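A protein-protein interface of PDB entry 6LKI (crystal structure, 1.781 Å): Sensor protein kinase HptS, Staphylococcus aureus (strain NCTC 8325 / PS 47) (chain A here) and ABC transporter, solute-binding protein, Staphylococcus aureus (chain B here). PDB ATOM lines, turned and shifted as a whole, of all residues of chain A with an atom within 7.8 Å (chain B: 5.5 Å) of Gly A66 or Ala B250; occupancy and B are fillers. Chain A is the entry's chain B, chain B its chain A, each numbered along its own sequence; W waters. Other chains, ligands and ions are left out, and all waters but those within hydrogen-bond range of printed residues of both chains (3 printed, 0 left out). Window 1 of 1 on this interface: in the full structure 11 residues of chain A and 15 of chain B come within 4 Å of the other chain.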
ATOM      1  N   LEU A  36       5.707   2.689  27.906  1.00  0.00           N
ATOM      2  CA  LEU A  36       4.300   2.651  28.287  1.00  0.00           C
ATOM      3  C   LEU A  36       4.083   2.629  29.796  1.00  0.00           C
ATOM      4  O   LEU A  36       2.933   2.518  30.236  1.00  0.00           O
ATOM      5  CB  LEU A  36       3.611   1.448  27.635  1.00  0.00           C
ATOM      6  CG  LEU A  36       3.568   1.497  26.104  1.00  0.00           C
ATOM      7  CD1 LEU A  36       2.576   0.487  25.547  1.00  0.00           C
ATOM      8  CD2 LEU A  36       3.238   2.904  25.613  1.00  0.00           C
ATOM      9  N   GLU A  63      -6.986  -3.701  21.436  1.00  0.00           N
ATOM     10  CA  GLU A  63      -6.554  -4.155  22.753  1.00  0.00           C
ATOM     11  C   GLU A  63      -5.033  -4.216  22.728  1.00  0.00           C
ATOM     12  O   GLU A  63      -4.454  -5.023  21.992  1.00  0.00           O
ATOM     13  CB  GLU A  63      -7.158  -5.516  23.107  1.00  0.00           C
ATOM     14  CG  GLU A  63      -8.648  -5.476  23.421  1.00  0.00           C
ATOM     15  CD  GLU A  63      -9.156  -6.775  24.024  1.00  0.00           C
ATOM     16  OE1 GLU A  63      -8.394  -7.763  24.044  1.00  0.00           O
ATOM     17  OE2 GLU A  63     -10.320  -6.807  24.480  1.00  0.00           O
ATOM     18  N   LEU A  64      -4.389  -3.346  23.499  1.00  0.00           N
ATOM     19  CA  LEU A  64      -2.936  -3.315  23.624  1.00  0.00           C
ATOM     20  C   LEU A  64      -2.587  -3.899  24.987  1.00  0.00           C
ATOM     21  O   LEU A  64      -2.813  -3.257  26.019  1.00  0.00           O
ATOM     22  CB  LEU A  64      -2.399  -1.893  23.470  1.00  0.00           C
ATOM     23  CG  LEU A  64      -0.881  -1.738  23.367  1.00  0.00           C
ATOM     24  CD1 LEU A  64      -0.335  -2.506  22.171  1.00  0.00           C
ATOM     25  CD2 LEU A  64      -0.502  -0.265  23.285  1.00  0.00           C
ATOM     26  N   SER A  65      -2.045  -5.113  24.990  1.00  0.00           N
ATOM     27  CA  SER A  65      -1.854  -5.885  26.211  1.00  0.00           C
ATOM     28  C   SER A  65      -0.371  -6.036  26.515  1.00  0.00           C
ATOM     29  O   SER A  65       0.409  -6.445  25.649  1.00  0.00           O
ATOM     30  CB  SER A  65      -2.509  -7.261  26.091  1.00  0.00           C
ATOM     31  OG  SER A  65      -3.887  -7.141  25.783  1.00  0.00           O
ATOM     32  N   GLY A  66       0.006  -5.714  27.749  1.00  0.00           N
ATOM     33  CA  GLY A  66       1.351  -5.928  28.223  1.00  0.00           C
ATOM     34  C   GLY A  66       1.341  -6.471  29.635  1.00  0.00           C
ATOM     35  O   GLY A  66       0.282  -6.744  30.207  1.00  0.00           O
ATOM     36  N   PRO A  67       2.529  -6.645  30.226  1.00  0.00           N
ATOM     37  CA  PRO A  67       2.600  -7.164  31.600  1.00  0.00           C
ATOM     38  C   PRO A  67       1.823  -6.308  32.589  1.00  0.00           C
ATOM     39  O   PRO A  67       2.226  -5.183  32.903  1.00  0.00           O
ATOM     40  CB  PRO A  67       4.106  -7.157  31.905  1.00  0.00           C
ATOM     41  CG  PRO A  67       4.724  -6.270  30.859  1.00  0.00           C
ATOM     42  CD  PRO A  67       3.862  -6.413  29.648  1.00  0.00           C
ATOM     43  N   ASN A  68       0.695  -6.840  33.068  1.00  0.00           N
ATOM     44  CA  ASN A  68      -0.170  -6.160  34.034  1.00  0.00           C
ATOM     45  C   ASN A  68      -0.656  -4.807  33.516  1.00  0.00           C
ATOM     46  O   ASN A  68      -0.834  -3.863  34.290  1.00  0.00           O
ATOM     47  CB  ASN A  68       0.531  -5.996  35.387  1.00  0.00           C
ATOM     48  CG  ASN A  68       0.774  -7.324  36.081  1.00  0.00           C
ATOM     49  OD1 ASN A  68      -0.021  -8.256  35.963  1.00  0.00           O
ATOM     50  ND2 ASN A  68       1.884  -7.419  36.807  1.00  0.00           N
ATOM     51  N   GLN A  69      -0.884  -4.706  32.206  1.00  0.00           N
ATOM     52  CA  GLN A  69      -1.319  -3.460  31.589  1.00  0.00           C
ATOM     53  C   GLN A  69      -2.273  -3.771  30.445  1.00  0.00           C
ATOM     54  O   GLN A  69      -2.020  -4.678  29.648  1.00  0.00           O
ATOM     55  CB  GLN A  69      -0.124  -2.647  31.081  1.00  0.00           C
ATOM     56  CG  GLN A  69      -0.432  -1.188  30.794  1.00  0.00           C
ATOM     57  CD  GLN A  69       0.824  -0.358  30.611  1.00  0.00           C
ATOM     58  OE1 GLN A  69       1.933  -0.891  30.566  1.00  0.00           O
ATOM     59  NE2 GLN A  69       0.657   0.956  30.509  1.00  0.00           N
ATOM     60  N   PHE A  70      -3.361  -3.007  30.365  1.00  0.00           N
ATOM     61  CA  PHE A  70      -4.415  -3.240  29.383  1.00  0.00           C
ATOM     62  C   PHE A  70      -4.916  -1.898  28.870  1.00  0.00           C
ATOM     63  O   PHE A  70      -5.482  -1.114  29.636  1.00  0.00           O
ATOM     64  CB  PHE A  70      -5.561  -4.051  30.003  1.00  0.00           C
ATOM     65  CG  PHE A  70      -6.623  -4.464  29.022  1.00  0.00           C
ATOM     66  CD1 PHE A  70      -6.335  -5.350  27.997  1.00  0.00           C
ATOM     67  CD2 PHE A  70      -7.914  -3.974  29.134  1.00  0.00           C
ATOM     68  CE1 PHE A  70      -7.315  -5.734  27.097  1.00  0.00           C
ATOM     69  CE2 PHE A  70      -8.897  -4.354  28.239  1.00  0.00           C
ATOM     70  CZ  PHE A  70      -8.596  -5.235  27.219  1.00  0.00           C
ATOM     71  N   ILE A  71      -4.710  -1.638  27.579  1.00  0.00           N
ATOM     72  CA  ILE A  71      -5.074  -0.375  26.944  1.00  0.00           C
ATOM     73  C   ILE A  71      -6.063  -0.678  25.827  1.00  0.00           C
ATOM     74  O   ILE A  71      -5.768  -1.480  24.932  1.00  0.00           O
ATOM     75  CB  ILE A  71      -3.839   0.363  26.400  1.00  0.00           C
ATOM     76  CG1 ILE A  71      -2.962   0.856  27.554  1.00  0.00           C
ATOM     77  CG2 ILE A  71      -4.250   1.518  25.494  1.00  0.00           C
ATOM     78  CD1 ILE A  71      -1.582   1.310  27.121  1.00  0.00           C
ATOM     79  N   GLN A  90       2.828  -8.430  17.445  1.00  0.00           N
ATOM     80  CA  GLN A  90       3.724  -8.438  18.597  1.00  0.00           C
ATOM     81  C   GLN A  90       4.670  -7.253  18.442  1.00  0.00           C
ATOM     82  O   GLN A  90       5.501  -7.230  17.527  1.00  0.00           O
ATOM     83  CB  GLN A  90       4.487  -9.759  18.690  1.00  0.00           C
ATOM     84  CG  GLN A  90       5.353  -9.893  19.933  1.00  0.00           C
ATOM     85  CD  GLN A  90       5.747 -11.332  20.223  1.00  0.00           C
ATOM     86  OE1 GLN A  90       5.099 -12.273  19.763  1.00  0.00           O
ATOM     87  NE2 GLN A  90       6.812 -11.508  20.997  1.00  0.00           N
ATOM     88  N   LEU A  91       4.540  -6.268  19.326  1.00  0.00           N
ATOM     89  CA  LEU A  91       5.215  -4.986  19.177  1.00  0.00           C
ATOM     90  C   LEU A  91       6.222  -4.779  20.298  1.00  0.00           C
ATOM     91  O   LEU A  91       5.927  -5.037  21.469  1.00  0.00           O
ATOM     92  CB  LEU A  91       4.206  -3.833  19.172  1.00  0.00           C
ATOM     93  CG  LEU A  91       3.071  -3.930  18.151  1.00  0.00           C
ATOM     94  CD1 LEU A  91       2.073  -2.799  18.358  1.00  0.00           C
ATOM     95  CD2 LEU A  91       3.622  -3.912  16.734  1.00  0.00           C
ATOM     96  N   ASN A  95       9.908  -0.275  26.952  1.00  0.00           N
ATOM     97  CA  ASN A  95       9.980  -0.931  28.252  1.00  0.00           C
ATOM     98  C   ASN A  95       9.711  -2.428  28.201  1.00  0.00           C
ATOM     99  O   ASN A  95      10.263  -3.168  29.021  1.00  0.00           O
ATOM    100  CB  ASN A  95       8.987  -0.287  29.223  1.00  0.00           C
ATOM    101  CG  ASN A  95       7.558  -0.366  28.725  1.00  0.00           C
ATOM    102  OD1 ASN A  95       7.272  -0.038  27.574  1.00  0.00           O
ATOM    103  ND2 ASN A  95       6.653  -0.812  29.591  1.00  0.00           N
ATOM    104  N   SER A  96       8.879  -2.891  27.276  1.00  0.00           N
ATOM    105  CA  SER A  96       8.477  -4.293  27.234  1.00  0.00           C
ATOM    106  C   SER A  96       7.822  -4.565  25.885  1.00  0.00           C
ATOM    107  O   SER A  96       7.667  -3.667  25.052  1.00  0.00           O
ATOM    108  CB  SER A  96       7.532  -4.633  28.390  1.00  0.00           C
ATOM    109  OG  SER A  96       7.169  -6.002  28.371  1.00  0.00           O
ATOM    110  N   THR A  97       7.439  -5.823  25.681  1.00  0.00           N
ATOM    111  CA  THR A  97       6.722  -6.242  24.485  1.00  0.00           C
ATOM    112  C   THR A  97       5.223  -6.224  24.761  1.00  0.00           C
ATOM    113  O   THR A  97       4.774  -6.699  25.809  1.00  0.00           O
ATOM    114  CB  THR A  97       7.170  -7.640  24.052  1.00  0.00           C
ATOM    115  OG1 THR A  97       8.422  -7.550  23.363  1.00  0.00           O
ATOM    116  CG2 THR A  97       6.139  -8.283  23.133  1.00  0.00           C
ATOM    117  N   TYR A  98       4.459  -5.669  23.827  1.00  0.00           N
ATOM    118  CA  TYR A  98       3.012  -5.584  23.941  1.00  0.00           C
ATOM    119  C   TYR A  98       2.361  -6.258  22.742  1.00  0.00           C
ATOM    120  O   TYR A  98       2.885  -6.216  21.625  1.00  0.00           O
ATOM    121  CB  TYR A  98       2.546  -4.125  24.036  1.00  0.00           C
ATOM    122  CG  TYR A  98       2.932  -3.439  25.330  1.00  0.00           C
ATOM    123  CD1 TYR A  98       4.245  -3.049  25.569  1.00  0.00           C
ATOM    124  CD2 TYR A  98       1.981  -3.176  26.308  1.00  0.00           C
ATOM    125  CE1 TYR A  98       4.599  -2.423  26.749  1.00  0.00           C
ATOM    126  CE2 TYR A  98       2.327  -2.553  27.491  1.00  0.00           C
ATOM    127  CZ  TYR A  98       3.636  -2.178  27.707  1.00  0.00           C
ATOM    128  OH  TYR A  98       3.981  -1.554  28.883  1.00  0.00           O
ATOM    129  N   MET A  99       1.217  -6.890  22.986  1.00  0.00           N
ATOM    130  CA  MET A  99       0.425  -7.510  21.932  1.00  0.00           C
ATOM    131  C   MET A  99      -0.706  -6.568  21.545  1.00  0.00           C
ATOM    132  O   MET A  99      -1.445  -6.090  22.411  1.00  0.00           O
ATOM    133  CB  MET A  99      -0.140  -8.857  22.386  1.00  0.00           C
ATOM    134  CG  MET A  99       0.911  -9.917  22.690  1.00  0.00           C
ATOM    135  SD  MET A  99       1.979 -10.290  21.282  1.00  0.00           S
ATOM    136  CE  MET A  99       0.772 -10.807  20.066  1.00  0.00           C
ATOM    137  N   LEU A 100      -0.835  -6.302  20.248  1.00  0.00           N
ATOM    138  CA  LEU A 100      -1.889  -5.445  19.722  1.00  0.00           C
ATOM    139  C   LEU A 100      -2.859  -6.296  18.915  1.00  0.00           C
ATOM    140  O   LEU A 100      -2.478  -6.881  17.897  1.00  0.00           O
ATOM    141  CB  LEU A 100      -1.313  -4.322  18.857  1.00  0.00           C
ATOM    142  CG  LEU A 100      -2.346  -3.451  18.137  1.00  0.00           C
ATOM    143  CD1 LEU A 100      -3.240  -2.732  19.140  1.00  0.00           C
ATOM    144  CD2 LEU A 100      -1.669  -2.454  17.202  1.00  0.00           C
ATOM    145  N   GLN B 245       7.955 -16.215  25.026  1.00  0.00           N
ATOM    146  CA  GLN B 245       7.839 -15.784  26.415  1.00  0.00           C
ATOM    147  C   GLN B 245       7.425 -14.321  26.514  1.00  0.00           C
ATOM    148  O   GLN B 245       6.694 -13.945  27.439  1.00  0.00           O
ATOM    149  CB  GLN B 245       9.161 -16.010  27.149  1.00  0.00           C
ATOM    150  CG  GLN B 245       9.443 -17.467  27.486  1.00  0.00           C
ATOM    151  CD  GLN B 245       8.871 -17.876  28.824  1.00  0.00           C
ATOM    152  OE1 GLN B 245       9.099 -17.213  29.836  1.00  0.00           O
ATOM    153  NE2 GLN B 245       8.125 -18.976  28.838  1.00  0.00           N
ATOM    154  N   GLN B 246       7.877 -13.484  25.577  1.00  0.00           N
ATOM    155  CA  GLN B 246       7.468 -12.082  25.580  1.00  0.00           C
ATOM    156  C   GLN B 246       5.974 -11.942  25.317  1.00  0.00           C
ATOM    157  O   GLN B 246       5.306 -11.099  25.931  1.00  0.00           O
ATOM    158  CB  GLN B 246       8.274 -11.299  24.544  1.00  0.00           C
ATOM    159  CG  GLN B 246       9.729 -11.088  24.928  1.00  0.00           C
ATOM    160  CD  GLN B 246      10.588 -10.673  23.750  1.00  0.00           C
ATOM    161  OE1 GLN B 246      10.296 -11.014  22.604  1.00  0.00           O
ATOM    162  NE2 GLN B 246      11.654  -9.932  24.028  1.00  0.00           N
ATOM    163  N   ARG B 247       5.429 -12.755  24.409  1.00  0.00           N
ATOM    164  CA  ARG B 247       3.991 -12.721  24.163  1.00  0.00           C
ATOM    165  C   ARG B 247       3.215 -13.269  25.355  1.00  0.00           C
ATOM    166  O   ARG B 247       2.164 -12.728  25.721  1.00  0.00           O
ATOM    167  CB  ARG B 247       3.653 -13.509  22.895  1.00  0.00           C
ATOM    168  CG  ARG B 247       2.158 -13.721  22.690  1.00  0.00           C
ATOM    169  CD  ARG B 247       1.833 -14.214  21.287  1.00  0.00           C
ATOM    170  NE  ARG B 247       0.390 -14.310  21.077  1.00  0.00           N
ATOM    171  CZ  ARG B 247      -0.185 -14.558  19.904  1.00  0.00           C
ATOM    172  NH1 ARG B 247       0.561 -14.735  18.821  1.00  0.00           N
ATOM    173  NH2 ARG B 247      -1.506 -14.626  19.814  1.00  0.00           N
ATOM    174  N   LEU B 248       3.722 -14.337  25.976  1.00  0.00           N
ATOM    175  CA  LEU B 248       3.027 -14.934  27.113  1.00  0.00           C
ATOM    176  C   LEU B 248       2.971 -13.977  28.297  1.00  0.00           C
ATOM    177  O   LEU B 248       1.947 -13.890  28.985  1.00  0.00           O
ATOM    178  CB  LEU B 248       3.707 -16.243  27.512  1.00  0.00           C
ATOM    179  CG  LEU B 248       3.417 -17.442  26.610  1.00  0.00           C
ATOM    180  CD1 LEU B 248       4.513 -18.485  26.740  1.00  0.00           C
ATOM    181  CD2 LEU B 248       2.060 -18.041  26.944  1.00  0.00           C
ATOM    182  N   VAL B 249       4.065 -13.256  28.554  1.00  0.00           N
ATOM    183  CA  VAL B 249       4.073 -12.285  29.648  1.00  0.00           C
ATOM    184  C   VAL B 249       3.019 -11.210  29.411  1.00  0.00           C
ATOM    185  O   VAL B 249       2.303 -10.803  30.337  1.00  0.00           O
ATOM    186  CB  VAL B 249       5.482 -11.682  29.809  1.00  0.00           C
ATOM    187  CG1 VAL B 249       5.429 -10.384  30.599  1.00  0.00           C
ATOM    188  CG2 VAL B 249       6.410 -12.681  30.487  1.00  0.00           C
ATOM    189  N   ALA B 250       2.889 -10.752  28.165  1.00  0.00           N
ATOM    190  CA  ALA B 250       1.929  -9.695  27.860  1.00  0.00           C
ATOM    191  C   ALA B 250       0.490 -10.187  27.946  1.00  0.00           C
ATOM    192  O   ALA B 250      -0.398  -9.426  28.346  1.00  0.00           O
ATOM    193  CB  ALA B 250       2.206  -9.122  26.471  1.00  0.00           C
ATOM    194  N   GLU B 251       0.235 -11.442  27.581  1.00  0.00           N
ATOM    195  CA  GLU B 251      -1.138 -11.927  27.509  1.00  0.00           C
ATOM    196  C   GLU B 251      -1.608 -12.574  28.806  1.00  0.00           C
ATOM    197  O   GLU B 251      -2.778 -12.425  29.180  1.00  0.00           O
ATOM    198  CB  GLU B 251      -1.282 -12.918  26.351  1.00  0.00           C
ATOM    199  CG  GLU B 251      -1.035 -12.300  24.982  1.00  0.00           C
ATOM    200  CD  GLU B 251      -1.447 -13.212  23.842  1.00  0.00           C
ATOM    201  OE1 GLU B 251      -1.660 -14.419  24.084  1.00  0.00           O
ATOM    202  OE2 GLU B 251      -1.562 -12.717  22.702  1.00  0.00           O
ATOM    203  N   PHE B 252      -0.724 -13.283  29.504  1.00  0.00           N
ATOM    204  CA  PHE B 252      -1.087 -13.993  30.724  1.00  0.00           C
ATOM    205  C   PHE B 252      -0.910 -13.154  31.982  1.00  0.00           C
ATOM    206  O   PHE B 252      -1.301 -13.607  33.063  1.00  0.00           O
ATOM    207  CB  PHE B 252      -0.250 -15.271  30.876  1.00  0.00           C
ATOM    208  CG  PHE B 252      -0.699 -16.415  30.006  1.00  0.00           C
ATOM    209  CD1 PHE B 252      -1.404 -16.192  28.835  1.00  0.00           C
ATOM    210  CD2 PHE B 252      -0.400 -17.719  30.361  1.00  0.00           C
ATOM    211  CE1 PHE B 252      -1.805 -17.248  28.038  1.00  0.00           C
ATOM    212  CE2 PHE B 252      -0.799 -18.779  29.570  1.00  0.00           C
ATOM    213  CZ  PHE B 252      -1.502 -18.543  28.408  1.00  0.00           C
ATOM    214  N   ASP B 253      -0.327 -11.959  31.870  1.00  0.00           N
ATOM    215  CA  ASP B 253       0.068 -11.167  33.035  1.00  0.00           C
ATOM    216  C   ASP B 253       0.959 -11.988  33.964  1.00  0.00           C
ATOM    217  O   ASP B 253       0.839 -11.942  35.191  1.00  0.00           O
ATOM    218  CB  ASP B 253      -1.152 -10.619  33.775  1.00  0.00           C
ATOM    219  CG  ASP B 253      -1.860  -9.538  32.990  1.00  0.00           C
ATOM    220  OD1 ASP B 253      -1.167  -8.765  32.295  1.00  0.00           O
ATOM    221  OD2 ASP B 253      -3.105  -9.462  33.062  1.00  0.00           O
HETATM  222  O   HOH W   1       5.828  -8.756  27.290  1.00  0.00           O
HETATM  223  O   HOH W   2       3.209 -13.238  17.915  1.00  0.00           O
HETATM  224  O   HOH W   3       8.732  -9.364  21.210  1.00  0.00           O
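Gly A66 touches just these residues of chain B: Ala B250 and Asp B253.
Ala B250 touches four residues of chain A.
Of the printed residues of chain B, Ser A65 touches Ala B250 (3.3 Å).
Printed residues of chain B within 4 Å of Pro A67: Val B249 (3.7 Å), Ala B250 (3.9 Å) and Asp B253 (3.9 Å).
Of the printed residues of chain B, Gln A90 touches Gln B246 and Arg B247.
Printed residues of chain A within 4 Å of Val B249: Pro A67.
Ile A71 touches none of the printed residues of chain B.
OE2 of Glu B251 lies within salt-bridge range of NE of Arg B247, at 3.0 Å.
O of Ser A65 sits at hydrogen-bond distance from N of Met A99 (2.8 Å).
Water W3 lies within hydrogen-bond range of OE1 of Gln B246 (2.7 Å), OG1 of Thr A97 (2.8 Å) and NE2 of Gln A90 (2.9 Å).
Water W1 lies within hydrogen-bond range of the backbone carbonyl oxygen (O) of Thr A97 (2.7 Å), the backbone carbonyl oxygen (O) of Gln B246 (2.8 Å) and the side-chain hydroxyl (OG) of Ser A96 (3.2 Å).
Water W2 lies within hydrogen-bond range of OE1 of Gln A90 and NH1 of Arg B247.
O of Gly A66 sits close to O of Ala B250, at 3.3 Å.
N of Asn A68 lies within hydrogen-bond range of OD1 of Asp B253 (2.8 Å).
O of Gly A66 sits close to OD1 of Asp B253, at 3.2 Å.
Printed residues of chain B that touch a printed residue of chain A: Gln B246, Arg B247, Val B249, Ala B250, Glu B251 and Asp B253.
Hydrophobic or aromatic side chains of chain B that line the printed part of chain A: Val B249 and Ala B250.
Among the printed residues, pairs that only touch across the chains: Ser A65 with Ala B250 (3.3 Å), Thr A97 with Ala B250 (3.6 Å), Gln A90 with Arg B247 (3.7 Å), Met A99 with Arg B247 (3.7 Å), Pro A67 with Val B249 (3.7 Å), Met A99 with Glu B251 (3.7 Å), Thr A97 with Gln B246 (3.8 Å), Gln A90 with Gln B246 (3.8 Å), Pro A67 with Asp B253 (3.9 Å) and Pro A67 with Ala B250 (3.9 Å).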
